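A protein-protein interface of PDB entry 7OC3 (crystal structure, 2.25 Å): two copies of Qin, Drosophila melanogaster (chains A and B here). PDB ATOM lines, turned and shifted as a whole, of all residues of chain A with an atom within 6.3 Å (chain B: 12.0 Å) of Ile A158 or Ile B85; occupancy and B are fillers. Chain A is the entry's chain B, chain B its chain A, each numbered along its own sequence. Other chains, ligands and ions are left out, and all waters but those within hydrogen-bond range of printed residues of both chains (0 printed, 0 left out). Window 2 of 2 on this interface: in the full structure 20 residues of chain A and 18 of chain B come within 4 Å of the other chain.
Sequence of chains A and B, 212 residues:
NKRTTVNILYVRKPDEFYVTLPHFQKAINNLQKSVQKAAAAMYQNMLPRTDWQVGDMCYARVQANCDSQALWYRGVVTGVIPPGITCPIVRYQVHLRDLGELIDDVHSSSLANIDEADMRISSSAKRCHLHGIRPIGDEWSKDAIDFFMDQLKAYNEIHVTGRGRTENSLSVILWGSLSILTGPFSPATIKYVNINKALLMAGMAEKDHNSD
The side-chain amino group of Lys A153 is in hydrogen-bond range of the backbone carbonyl oxygen of Pro B83.
The backbone carbonyl oxygen (O) of Ile A158 is in hydrogen-bond range of the backbone NH (N) of Val A6, at 3.0 Å.
CG1 of Ile A8 touches CD1 of Ile B85, 3.5 Å away. Ile B85 touches Leu A152. Ile A158 touches Ile B85 (CG1 to CD1, 3.97 Å).
Of the printed residues of chain B, Ile A158 touches Ile B85 (3.97 Å). Ile B85 touches just these residues of chain A: Ile A8, Leu A152 and Ile A158. No residue of chain B comes within 4 Å of Val A6. Ile A8 touches just one residue of chain B: Ile B85. No residue of chain B comes within 4 Å of Met A149. Of chain B, only Ile B85 (3.5 Å) comes within 4 Å of Leu A152. Lys A153 touches just one residue of chain B: Pro B83. No residue of chain B comes within 4 Å of Glu A157. No residue of chain B comes within 4 Å of His A159. No residue of chain B comes within 4 Å of Val A160. No residue of chain B comes within 4 Å of Leu A174. No residue of chain B comes within 4 Å of Gly A176. Printed residues of chain A within 4 Å of Pro B83: Lys A153 (3.0 Å). Val A11 touches none of the printed residues of chain B. Tyr A155 touches none of the printed residues of chain B. The nearest residue of chain B that does not touch Ile A158 is Thr B86 (9.1 Å). The nearest printed residue of chain A that does not touch Pro B83 is Met A149 (7.1 Å).
Hydrophobic or aromatic side chains of chain A that line the printed part of chain B: Ile A8, Leu A152 and Ile A158. Of the 12 printed residues of chain B, 2 touch a printed residue of chain A. Among the printed residues, 4 pairs touch across the chains. Among the printed residues, no Asp or Glu carboxylate lies within 4 Å of a Lys or Arg side-chain nitrogen of the other chain.
No position is printed for both chains. Of the 4 pairs that touch across the chains among the printed residues, none has its exchanged pair printed and touching as well.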
ATOM      1  N   THR A   4      15.891  -6.621 -33.769  1.00  0.00           N
ATOM      2  CA  THR A   4      15.406  -6.527 -32.399  1.00  0.00           C
ATOM      3  C   THR A   4      15.280  -7.921 -31.780  1.00  0.00           C
ATOM      4  O   THR A   4      14.659  -8.810 -32.362  1.00  0.00           O
ATOM      5  CB  THR A   4      14.049  -5.799 -32.323  1.00  0.00           C
ATOM      6  OG1 THR A   4      12.992  -6.707 -32.657  1.00  0.00           O
ATOM      7  CG2 THR A   4      14.018  -4.610 -33.275  1.00  0.00           C
ATOM      8  N   THR A   5      15.877  -8.116 -30.609  1.00  0.00           N
ATOM      9  CA  THR A   5      15.828  -9.413 -29.944  1.00  0.00           C
ATOM     10  C   THR A   5      14.403  -9.682 -29.462  1.00  0.00           C
ATOM     11  O   THR A   5      13.697  -8.753 -29.071  1.00  0.00           O
ATOM     12  CB  THR A   5      16.818  -9.475 -28.762  1.00  0.00           C
ATOM     13  OG1 THR A   5      18.103  -9.018 -29.200  1.00  0.00           O
ATOM     14  CG2 THR A   5      16.952 -10.897 -28.228  1.00  0.00           C
ATOM     15  N   VAL A   6      13.958 -10.935 -29.542  1.00  0.00           N
ATOM     16  CA  VAL A   6      12.614 -11.290 -29.076  1.00  0.00           C
ATOM     17  C   VAL A   6      12.602 -12.598 -28.305  1.00  0.00           C
ATOM     18  O   VAL A   6      13.527 -13.406 -28.394  1.00  0.00           O
ATOM     19  CB  VAL A   6      11.599 -11.434 -30.231  1.00  0.00           C
ATOM     20  CG1 VAL A   6      11.421 -10.118 -30.971  1.00  0.00           C
ATOM     21  CG2 VAL A   6      12.026 -12.544 -31.175  1.00  0.00           C
ATOM     22  N   ASN A   7      11.535 -12.794 -27.543  1.00  0.00           N
ATOM     23  CA  ASN A   7      11.277 -14.072 -26.904  1.00  0.00           C
ATOM     24  C   ASN A   7      10.204 -14.800 -27.707  1.00  0.00           C
ATOM     25  O   ASN A   7       9.178 -14.212 -28.048  1.00  0.00           O
ATOM     26  CB  ASN A   7      10.817 -13.879 -25.456  1.00  0.00           C
ATOM     27  CG  ASN A   7      11.947 -13.455 -24.522  1.00  0.00           C
ATOM     28  OD1 ASN A   7      13.117 -13.761 -24.753  1.00  0.00           O
ATOM     29  ND2 ASN A   7      11.593 -12.742 -23.461  1.00  0.00           N
ATOM     30  N   ILE A   8      10.445 -16.063 -28.037  1.00  0.00           N
ATOM     31  CA  ILE A   8       9.443 -16.862 -28.734  1.00  0.00           C
ATOM     32  C   ILE A   8       8.452 -17.479 -27.743  1.00  0.00           C
ATOM     33  O   ILE A   8       8.812 -18.363 -26.967  1.00  0.00           O
ATOM     34  CB  ILE A   8      10.089 -17.972 -29.577  1.00  0.00           C
ATOM     35  CG1 ILE A   8      11.194 -17.385 -30.460  1.00  0.00           C
ATOM     36  CG2 ILE A   8       9.039 -18.671 -30.434  1.00  0.00           C
ATOM     37  CD1 ILE A   8      10.682 -16.618 -31.656  1.00  0.00           C
ATOM     38  N   VAL A  11       4.898 -21.459 -31.087  1.00  0.00           N
ATOM     39  CA  VAL A  11       5.018 -21.678 -32.524  1.00  0.00           C
ATOM     40  C   VAL A  11       3.972 -22.671 -33.047  1.00  0.00           C
ATOM     41  O   VAL A  11       3.866 -23.796 -32.560  1.00  0.00           O
ATOM     42  CB  VAL A  11       6.414 -22.195 -32.900  1.00  0.00           C
ATOM     43  CG1 VAL A  11       6.496 -22.452 -34.401  1.00  0.00           C
ATOM     44  CG2 VAL A  11       7.478 -21.194 -32.488  1.00  0.00           C
ATOM     45  N   MET A 149      11.279 -25.617 -35.707  1.00  0.00           N
ATOM     46  CA  MET A 149      11.470 -25.733 -34.258  1.00  0.00           C
ATOM     47  C   MET A 149      12.921 -26.007 -33.888  1.00  0.00           C
ATOM     48  O   MET A 149      13.433 -25.464 -32.908  1.00  0.00           O
ATOM     49  CB  MET A 149      10.586 -26.840 -33.679  1.00  0.00           C
ATOM     50  CG  MET A 149       9.105 -26.595 -33.854  1.00  0.00           C
ATOM     51  SD  MET A 149       8.568 -24.990 -32.907  1.00  0.00           S
ATOM     52  CE  MET A 149       8.935 -25.561 -31.079  1.00  0.00           C
ATOM     53  N   GLN A 151      15.597 -25.177 -35.579  1.00  0.00           N
ATOM     54  CA  GLN A 151      16.390 -23.975 -35.806  1.00  0.00           C
ATOM     55  C   GLN A 151      16.308 -23.028 -34.618  1.00  0.00           C
ATOM     56  O   GLN A 151      17.318 -22.468 -34.193  1.00  0.00           O
ATOM     57  CB  GLN A 151      15.935 -23.245 -37.073  1.00  0.00           C
ATOM     58  CG  GLN A 151      16.311 -23.934 -38.371  1.00  0.00           C
ATOM     59  CD  GLN A 151      17.792 -23.833 -38.665  1.00  0.00           C
ATOM     60  OE1 GLN A 151      18.368 -22.744 -38.655  1.00  0.00           O
ATOM     61  NE2 GLN A 151      18.420 -24.972 -38.933  1.00  0.00           N
ATOM     62  N   LEU A 152      15.107 -22.863 -34.076  1.00  0.00           N
ATOM     63  CA  LEU A 152      14.881 -21.898 -33.008  1.00  0.00           C
ATOM     64  C   LEU A 152      15.673 -22.229 -31.748  1.00  0.00           C
ATOM     65  O   LEU A 152      16.069 -21.334 -31.009  1.00  0.00           O
ATOM     66  CB  LEU A 152      13.393 -21.808 -32.673  1.00  0.00           C
ATOM     67  CG  LEU A 152      12.512 -21.271 -33.797  1.00  0.00           C
ATOM     68  CD1 LEU A 152      11.061 -21.271 -33.349  1.00  0.00           C
ATOM     69  CD2 LEU A 152      12.964 -19.884 -34.252  1.00  0.00           C
ATOM     70  N   LYS A 153      15.891 -23.513 -31.496  1.00  0.00           N
ATOM     71  CA  LYS A 153      16.615 -23.914 -30.299  1.00  0.00           C
ATOM     72  C   LYS A 153      18.105 -24.112 -30.557  1.00  0.00           C
ATOM     73  O   LYS A 153      18.867 -24.403 -29.642  1.00  0.00           O
ATOM     74  CB  LYS A 153      16.005 -25.187 -29.716  1.00  0.00           C
ATOM     75  CG  LYS A 153      16.194 -26.435 -30.553  1.00  0.00           C
ATOM     76  CD  LYS A 153      15.868 -27.661 -29.715  1.00  0.00           C
ATOM     77  CE  LYS A 153      15.308 -28.793 -30.553  1.00  0.00           C
ATOM     78  NZ  LYS A 153      14.226 -29.510 -29.815  1.00  0.00           N
ATOM     79  N   TYR A 155      20.187 -21.836 -31.531  1.00  0.00           N
ATOM     80  CA  TYR A 155      20.913 -20.574 -31.436  1.00  0.00           C
ATOM     81  C   TYR A 155      20.864 -19.958 -30.045  1.00  0.00           C
ATOM     82  O   TYR A 155      19.999 -20.279 -29.229  1.00  0.00           O
ATOM     83  CB  TYR A 155      20.376 -19.581 -32.467  1.00  0.00           C
ATOM     84  CG  TYR A 155      20.580 -20.062 -33.881  1.00  0.00           C
ATOM     85  CD1 TYR A 155      21.846 -20.087 -34.450  1.00  0.00           C
ATOM     86  CD2 TYR A 155      19.511 -20.509 -34.641  1.00  0.00           C
ATOM     87  CE1 TYR A 155      22.038 -20.539 -35.743  1.00  0.00           C
ATOM     88  CE2 TYR A 155      19.692 -20.962 -35.935  1.00  0.00           C
ATOM     89  CZ  TYR A 155      20.956 -20.976 -36.479  1.00  0.00           C
ATOM     90  OH  TYR A 155      21.138 -21.428 -37.762  1.00  0.00           O
ATOM     91  N   ASN A 156      21.819 -19.073 -29.787  1.00  0.00           N
ATOM     92  CA  ASN A 156      21.930 -18.379 -28.516  1.00  0.00           C
ATOM     93  C   ASN A 156      20.729 -17.472 -28.253  1.00  0.00           C
ATOM     94  O   ASN A 156      20.118 -17.527 -27.189  1.00  0.00           O
ATOM     95  CB  ASN A 156      23.229 -17.570 -28.496  1.00  0.00           C
ATOM     96  CG  ASN A 156      23.845 -17.492 -27.131  1.00  0.00           C
ATOM     97  OD1 ASN A 156      24.386 -18.476 -26.625  1.00  0.00           O
ATOM     98  ND2 ASN A 156      23.790 -16.314 -26.525  1.00  0.00           N
ATOM     99  N   GLU A 157      20.400 -16.631 -29.231  1.00  0.00           N
ATOM    100  CA  GLU A 157      19.255 -15.727 -29.127  1.00  0.00           C
ATOM    101  C   GLU A 157      18.516 -15.655 -30.457  1.00  0.00           C
ATOM    102  O   GLU A 157      19.039 -16.077 -31.487  1.00  0.00           O
ATOM    103  CB  GLU A 157      19.697 -14.327 -28.697  1.00  0.00           C
ATOM    104  CG  GLU A 157      20.214 -14.244 -27.263  1.00  0.00           C
ATOM    105  CD  GLU A 157      20.421 -12.815 -26.794  1.00  0.00           C
ATOM    106  OE1 GLU A 157      21.248 -12.099 -27.402  1.00  0.00           O
ATOM    107  OE2 GLU A 157      19.758 -12.408 -25.816  1.00  0.00           O
ATOM    108  N   ILE A 158      17.298 -15.125 -30.430  1.00  0.00           N
ATOM    109  CA  ILE A 158      16.502 -14.980 -31.646  1.00  0.00           C
ATOM    110  C   ILE A 158      16.185 -13.506 -31.874  1.00  0.00           C
ATOM    111  O   ILE A 158      15.887 -12.778 -30.927  1.00  0.00           O
ATOM    112  CB  ILE A 158      15.189 -15.797 -31.575  1.00  0.00           C
ATOM    113  CG1 ILE A 158      15.495 -17.267 -31.283  1.00  0.00           C
ATOM    114  CG2 ILE A 158      14.413 -15.690 -32.873  1.00  0.00           C
ATOM    115  CD1 ILE A 158      16.409 -17.910 -32.299  1.00  0.00           C
ATOM    116  N   HIS A 159      16.260 -13.070 -33.129  1.00  0.00           N
ATOM    117  CA  HIS A 159      16.027 -11.670 -33.472  1.00  0.00           C
ATOM    118  C   HIS A 159      15.148 -11.551 -34.708  1.00  0.00           C
ATOM    119  O   HIS A 159      15.167 -12.425 -35.577  1.00  0.00           O
ATOM    120  CB  HIS A 159      17.364 -10.949 -33.701  1.00  0.00           C
ATOM    121  CG  HIS A 159      18.445 -11.377 -32.758  1.00  0.00           C
ATOM    122  ND1 HIS A 159      18.742 -10.685 -31.602  1.00  0.00           N
ATOM    123  CD2 HIS A 159      19.287 -12.438 -32.787  1.00  0.00           C
ATOM    124  CE1 HIS A 159      19.724 -11.297 -30.965  1.00  0.00           C
ATOM    125  NE2 HIS A 159      20.073 -12.364 -31.664  1.00  0.00           N
ATOM    126  N   VAL A 160      14.388 -10.464 -34.795  1.00  0.00           N
ATOM    127  CA  VAL A 160      13.516 -10.243 -35.942  1.00  0.00           C
ATOM    128  C   VAL A 160      13.832  -8.939 -36.656  1.00  0.00           C
ATOM    129  O   VAL A 160      14.324  -7.980 -36.055  1.00  0.00           O
ATOM    130  CB  VAL A 160      12.020 -10.230 -35.539  1.00  0.00           C
ATOM    131  CG1 VAL A 160      11.723 -11.328 -34.542  1.00  0.00           C
ATOM    132  CG2 VAL A 160      11.624  -8.882 -34.960  1.00  0.00           C
ATOM    133  N   LEU A 174      13.614 -13.892 -39.498  1.00  0.00           N
ATOM    134  CA  LEU A 174      14.058 -14.386 -38.202  1.00  0.00           C
ATOM    135  C   LEU A 174      15.555 -14.671 -38.194  1.00  0.00           C
ATOM    136  O   LEU A 174      16.061 -15.348 -39.089  1.00  0.00           O
ATOM    137  CB  LEU A 174      13.275 -15.643 -37.823  1.00  0.00           C
ATOM    138  CG  LEU A 174      12.962 -15.786 -36.336  1.00  0.00           C
ATOM    139  CD1 LEU A 174      12.335 -14.509 -35.837  1.00  0.00           C
ATOM    140  CD2 LEU A 174      12.029 -16.953 -36.100  1.00  0.00           C
ATOM    141  N   TRP A 175      16.253 -14.162 -37.181  1.00  0.00           N
ATOM    142  CA  TRP A 175      17.702 -14.334 -37.082  1.00  0.00           C
ATOM    143  C   TRP A 175      18.099 -15.160 -35.868  1.00  0.00           C
ATOM    144  O   TRP A 175      17.607 -14.933 -34.767  1.00  0.00           O
ATOM    145  CB  TRP A 175      18.410 -12.973 -37.009  1.00  0.00           C
ATOM    146  CG  TRP A 175      18.235 -12.110 -38.218  1.00  0.00           C
ATOM    147  CD1 TRP A 175      17.290 -11.145 -38.404  1.00  0.00           C
ATOM    148  CD2 TRP A 175      19.044 -12.112 -39.402  1.00  0.00           C
ATOM    149  NE1 TRP A 175      17.447 -10.556 -39.637  1.00  0.00           N
ATOM    150  CE2 TRP A 175      18.518 -11.132 -40.269  1.00  0.00           C
ATOM    151  CE3 TRP A 175      20.156 -12.854 -39.816  1.00  0.00           C
ATOM    152  CZ2 TRP A 175      19.061 -10.877 -41.527  1.00  0.00           C
ATOM    153  CZ3 TRP A 175      20.699 -12.596 -41.067  1.00  0.00           C
ATOM    154  CH2 TRP A 175      20.150 -11.615 -41.906  1.00  0.00           C
ATOM    155  N   GLY A 176      19.017 -16.098 -36.071  1.00  0.00           N
ATOM    156  CA  GLY A 176      19.614 -16.819 -34.965  1.00  0.00           C
ATOM    157  C   GLY A 176      21.017 -16.292 -34.722  1.00  0.00           C
ATOM    158  O   GLY A 176      21.763 -16.059 -35.667  1.00  0.00           O
ATOM    159  N   SER A 177      21.381 -16.102 -33.460  1.00  0.00           N
ATOM    160  CA  SER A 177      22.707 -15.579 -33.140  1.00  0.00           C
ATOM    161  C   SER A 177      23.575 -16.595 -32.414  1.00  0.00           C
ATOM    162  O   SER A 177      23.107 -17.310 -31.531  1.00  0.00           O
ATOM    163  CB  SER A 177      22.593 -14.312 -32.294  1.00  0.00           C
ATOM    164  OG  SER A 177      21.970 -14.588 -31.051  1.00  0.00           O
ATOM    165  N   ILE A 195      17.343 -17.546 -40.519  1.00  0.00           N
ATOM    166  CA  ILE A 195      16.525 -18.748 -40.378  1.00  0.00           C
ATOM    167  C   ILE A 195      15.584 -18.944 -41.573  1.00  0.00           C
ATOM    168  O   ILE A 195      15.379 -20.076 -42.017  1.00  0.00           O
ATOM    169  CB  ILE A 195      15.720 -18.715 -39.068  1.00  0.00           C
ATOM    170  CG1 ILE A 195      16.673 -18.817 -37.874  1.00  0.00           C
ATOM    171  CG2 ILE A 195      14.727 -19.854 -39.015  1.00  0.00           C
ATOM    172  CD1 ILE A 195      16.229 -18.030 -36.668  1.00  0.00           C
ATOM    173  N   ILE B  81       9.226 -36.237 -26.232  1.00  0.00           N
ATOM    174  CA  ILE B  81       9.329 -34.933 -26.871  1.00  0.00           C
ATOM    175  C   ILE B  81      10.423 -34.103 -26.203  1.00  0.00           C
ATOM    176  O   ILE B  81      10.247 -33.622 -25.078  1.00  0.00           O
ATOM    177  CB  ILE B  81       7.989 -34.177 -26.812  1.00  0.00           C
ATOM    178  CG1 ILE B  81       6.890 -34.987 -27.507  1.00  0.00           C
ATOM    179  CG2 ILE B  81       8.121 -32.804 -27.445  1.00  0.00           C
ATOM    180  CD1 ILE B  81       5.545 -34.944 -26.810  1.00  0.00           C
ATOM    181  N   PRO B  82      11.545 -33.900 -26.914  1.00  0.00           N
ATOM    182  CA  PRO B  82      12.710 -33.222 -26.336  1.00  0.00           C
ATOM    183  C   PRO B  82      12.394 -31.775 -26.008  1.00  0.00           C
ATOM    184  O   PRO B  82      11.463 -31.219 -26.586  1.00  0.00           O
ATOM    185  CB  PRO B  82      13.761 -33.321 -27.447  1.00  0.00           C
ATOM    186  CG  PRO B  82      12.960 -33.380 -28.706  1.00  0.00           C
ATOM    187  CD  PRO B  82      11.719 -34.168 -28.352  1.00  0.00           C
ATOM    188  N   PRO B  83      13.149 -31.175 -25.076  1.00  0.00           N
ATOM    189  CA  PRO B  83      12.921 -29.769 -24.735  1.00  0.00           C
ATOM    190  C   PRO B  83      13.019 -28.885 -25.972  1.00  0.00           C
ATOM    191  O   PRO B  83      13.748 -29.216 -26.906  1.00  0.00           O
ATOM    192  CB  PRO B  83      14.045 -29.461 -23.745  1.00  0.00           C
ATOM    193  CG  PRO B  83      14.383 -30.784 -23.149  1.00  0.00           C
ATOM    194  CD  PRO B  83      14.225 -31.771 -24.270  1.00  0.00           C
ATOM    195  N   GLY B  84      12.257 -27.799 -25.986  1.00  0.00           N
ATOM    196  CA  GLY B  84      12.255 -26.882 -27.106  1.00  0.00           C
ATOM    197  C   GLY B  84      12.339 -25.454 -26.619  1.00  0.00           C
ATOM    198  O   GLY B  84      12.329 -25.202 -25.415  1.00  0.00           O
ATOM    199  N   ILE B  85      12.396 -24.519 -27.558  1.00  0.00           N
ATOM    200  CA  ILE B  85      12.538 -23.105 -27.232  1.00  0.00           C
ATOM    201  C   ILE B  85      11.343 -22.575 -26.440  1.00  0.00           C
ATOM    202  O   ILE B  85      11.504 -21.773 -25.519  1.00  0.00           O
ATOM    203  CB  ILE B  85      12.736 -22.264 -28.517  1.00  0.00           C
ATOM    204  CG1 ILE B  85      12.743 -20.769 -28.189  1.00  0.00           C
ATOM    205  CG2 ILE B  85      11.662 -22.585 -29.554  1.00  0.00           C
ATOM    206  CD1 ILE B  85      13.332 -19.924 -29.277  1.00  0.00           C
ATOM    207  N   THR B  86      10.150 -23.033 -26.801  1.00  0.00           N
ATOM    208  CA  THR B  86       8.925 -22.663 -26.102  1.00  0.00           C
ATOM    209  C   THR B  86       8.770 -23.392 -24.764  1.00  0.00           C
ATOM    210  O   THR B  86       8.214 -22.842 -23.815  1.00  0.00           O
ATOM    211  CB  THR B  86       7.696 -22.940 -26.974  1.00  0.00           C
ATOM    212  OG1 THR B  86       7.717 -24.308 -27.396  1.00  0.00           O
ATOM    213  CG2 THR B  86       7.712 -22.038 -28.198  1.00  0.00           C
ATOM    214  N   CYS B  87       9.217 -24.643 -24.705  1.00  0.00           N
ATOM    215  CA  CYS B  87       9.080 -25.446 -23.491  1.00  0.00           C
ATOM    216  C   CYS B  87      10.357 -26.218 -23.167  1.00  0.00           C
ATOM    217  O   CYS B  87      10.675 -27.207 -23.829  1.00  0.00           O
ATOM    218  CB  CYS B  87       7.903 -26.418 -23.629  1.00  0.00           C
ATOM    219  SG  CYS B  87       7.537 -27.373 -22.136  1.00  0.00           S
ATOM    220  N   PRO B  88      11.079 -25.784 -22.122  1.00  0.00           N
ATOM    221  CA  PRO B  88      12.422 -26.284 -21.809  1.00  0.00           C
ATOM    222  C   PRO B  88      12.450 -27.585 -21.001  1.00  0.00           C
ATOM    223  O   PRO B  88      13.477 -27.885 -20.392  1.00  0.00           O
ATOM    224  CB  PRO B  88      13.036 -25.138 -21.003  1.00  0.00           C
ATOM    225  CG  PRO B  88      11.882 -24.453 -20.367  1.00  0.00           C
ATOM    226  CD  PRO B  88      10.656 -24.713 -21.204  1.00  0.00           C
ATOM    227  N   ILE B  89      11.349 -28.333 -20.995  1.00  0.00           N
ATOM    228  CA  ILE B  89      11.286 -29.608 -20.282  1.00  0.00           C
ATOM    229  C   ILE B  89      11.019 -30.748 -21.260  1.00  0.00           C
ATOM    230  O   ILE B  89      10.331 -30.561 -22.264  1.00  0.00           O
ATOM    231  CB  ILE B  89      10.173 -29.615 -19.209  1.00  0.00           C
ATOM    232  CG1 ILE B  89      10.113 -28.273 -18.478  1.00  0.00           C
ATOM    233  CG2 ILE B  89      10.365 -30.771 -18.232  1.00  0.00           C
ATOM    234  CD1 ILE B  89       9.028 -28.208 -17.421  1.00  0.00           C
ATOM    235  N   VAL B  90      11.543 -31.933 -20.961  1.00  0.00           N
ATOM    236  CA  VAL B  90      11.160 -33.123 -21.706  1.00  0.00           C
ATOM    237  C   VAL B  90       9.687 -33.412 -21.441  1.00  0.00           C
ATOM    238  O   VAL B  90       9.202 -33.228 -20.326  1.00  0.00           O
ATOM    239  CB  VAL B  90      12.017 -34.348 -21.327  1.00  0.00           C
ATOM    240  CG1 VAL B  90      11.932 -34.621 -19.835  1.00  0.00           C
ATOM    241  CG2 VAL B  90      11.590 -35.572 -22.124  1.00  0.00           C
ATOM    242  N   ARG B  91       8.974 -33.834 -22.477  1.00  0.00           N
ATOM    243  CA  ARG B  91       7.566 -34.187 -22.350  1.00  0.00           C
ATOM    244  C   ARG B  91       7.330 -35.510 -23.052  1.00  0.00           C
ATOM    245  O   ARG B  91       8.233 -36.031 -23.710  1.00  0.00           O
ATOM    246  CB  ARG B  91       6.676 -33.089 -22.924  1.00  0.00           C
ATOM    247  CG  ARG B  91       6.553 -31.876 -22.020  1.00  0.00           C
ATOM    248  CD  ARG B  91       5.848 -30.743 -22.733  1.00  0.00           C
ATOM    249  NE  ARG B  91       6.446 -30.497 -24.040  1.00  0.00           N
ATOM    250  CZ  ARG B  91       6.045 -29.549 -24.880  1.00  0.00           C
ATOM    251  NH1 ARG B  91       5.037 -28.754 -24.552  1.00  0.00           N
ATOM    252  NH2 ARG B  91       6.654 -29.399 -26.051  1.00  0.00           N
ATOM    253  N   ASP B 105       2.305 -33.712 -25.178  1.00  0.00           N
ATOM    254  CA  ASP B 105       2.760 -32.711 -24.210  1.00  0.00           C
ATOM    255  C   ASP B 105       2.420 -33.076 -22.767  1.00  0.00           C
ATOM    256  O   ASP B 105       1.959 -32.237 -21.987  1.00  0.00           O
ATOM    257  CB  ASP B 105       2.166 -31.341 -24.544  1.00  0.00           C
ATOM    258  CG  ASP B 105       2.531 -30.868 -25.941  1.00  0.00           C
ATOM    259  OD1 ASP B 105       3.547 -31.351 -26.488  1.00  0.00           O
ATOM    260  OD2 ASP B 105       1.809 -30.003 -26.482  1.00  0.00           O
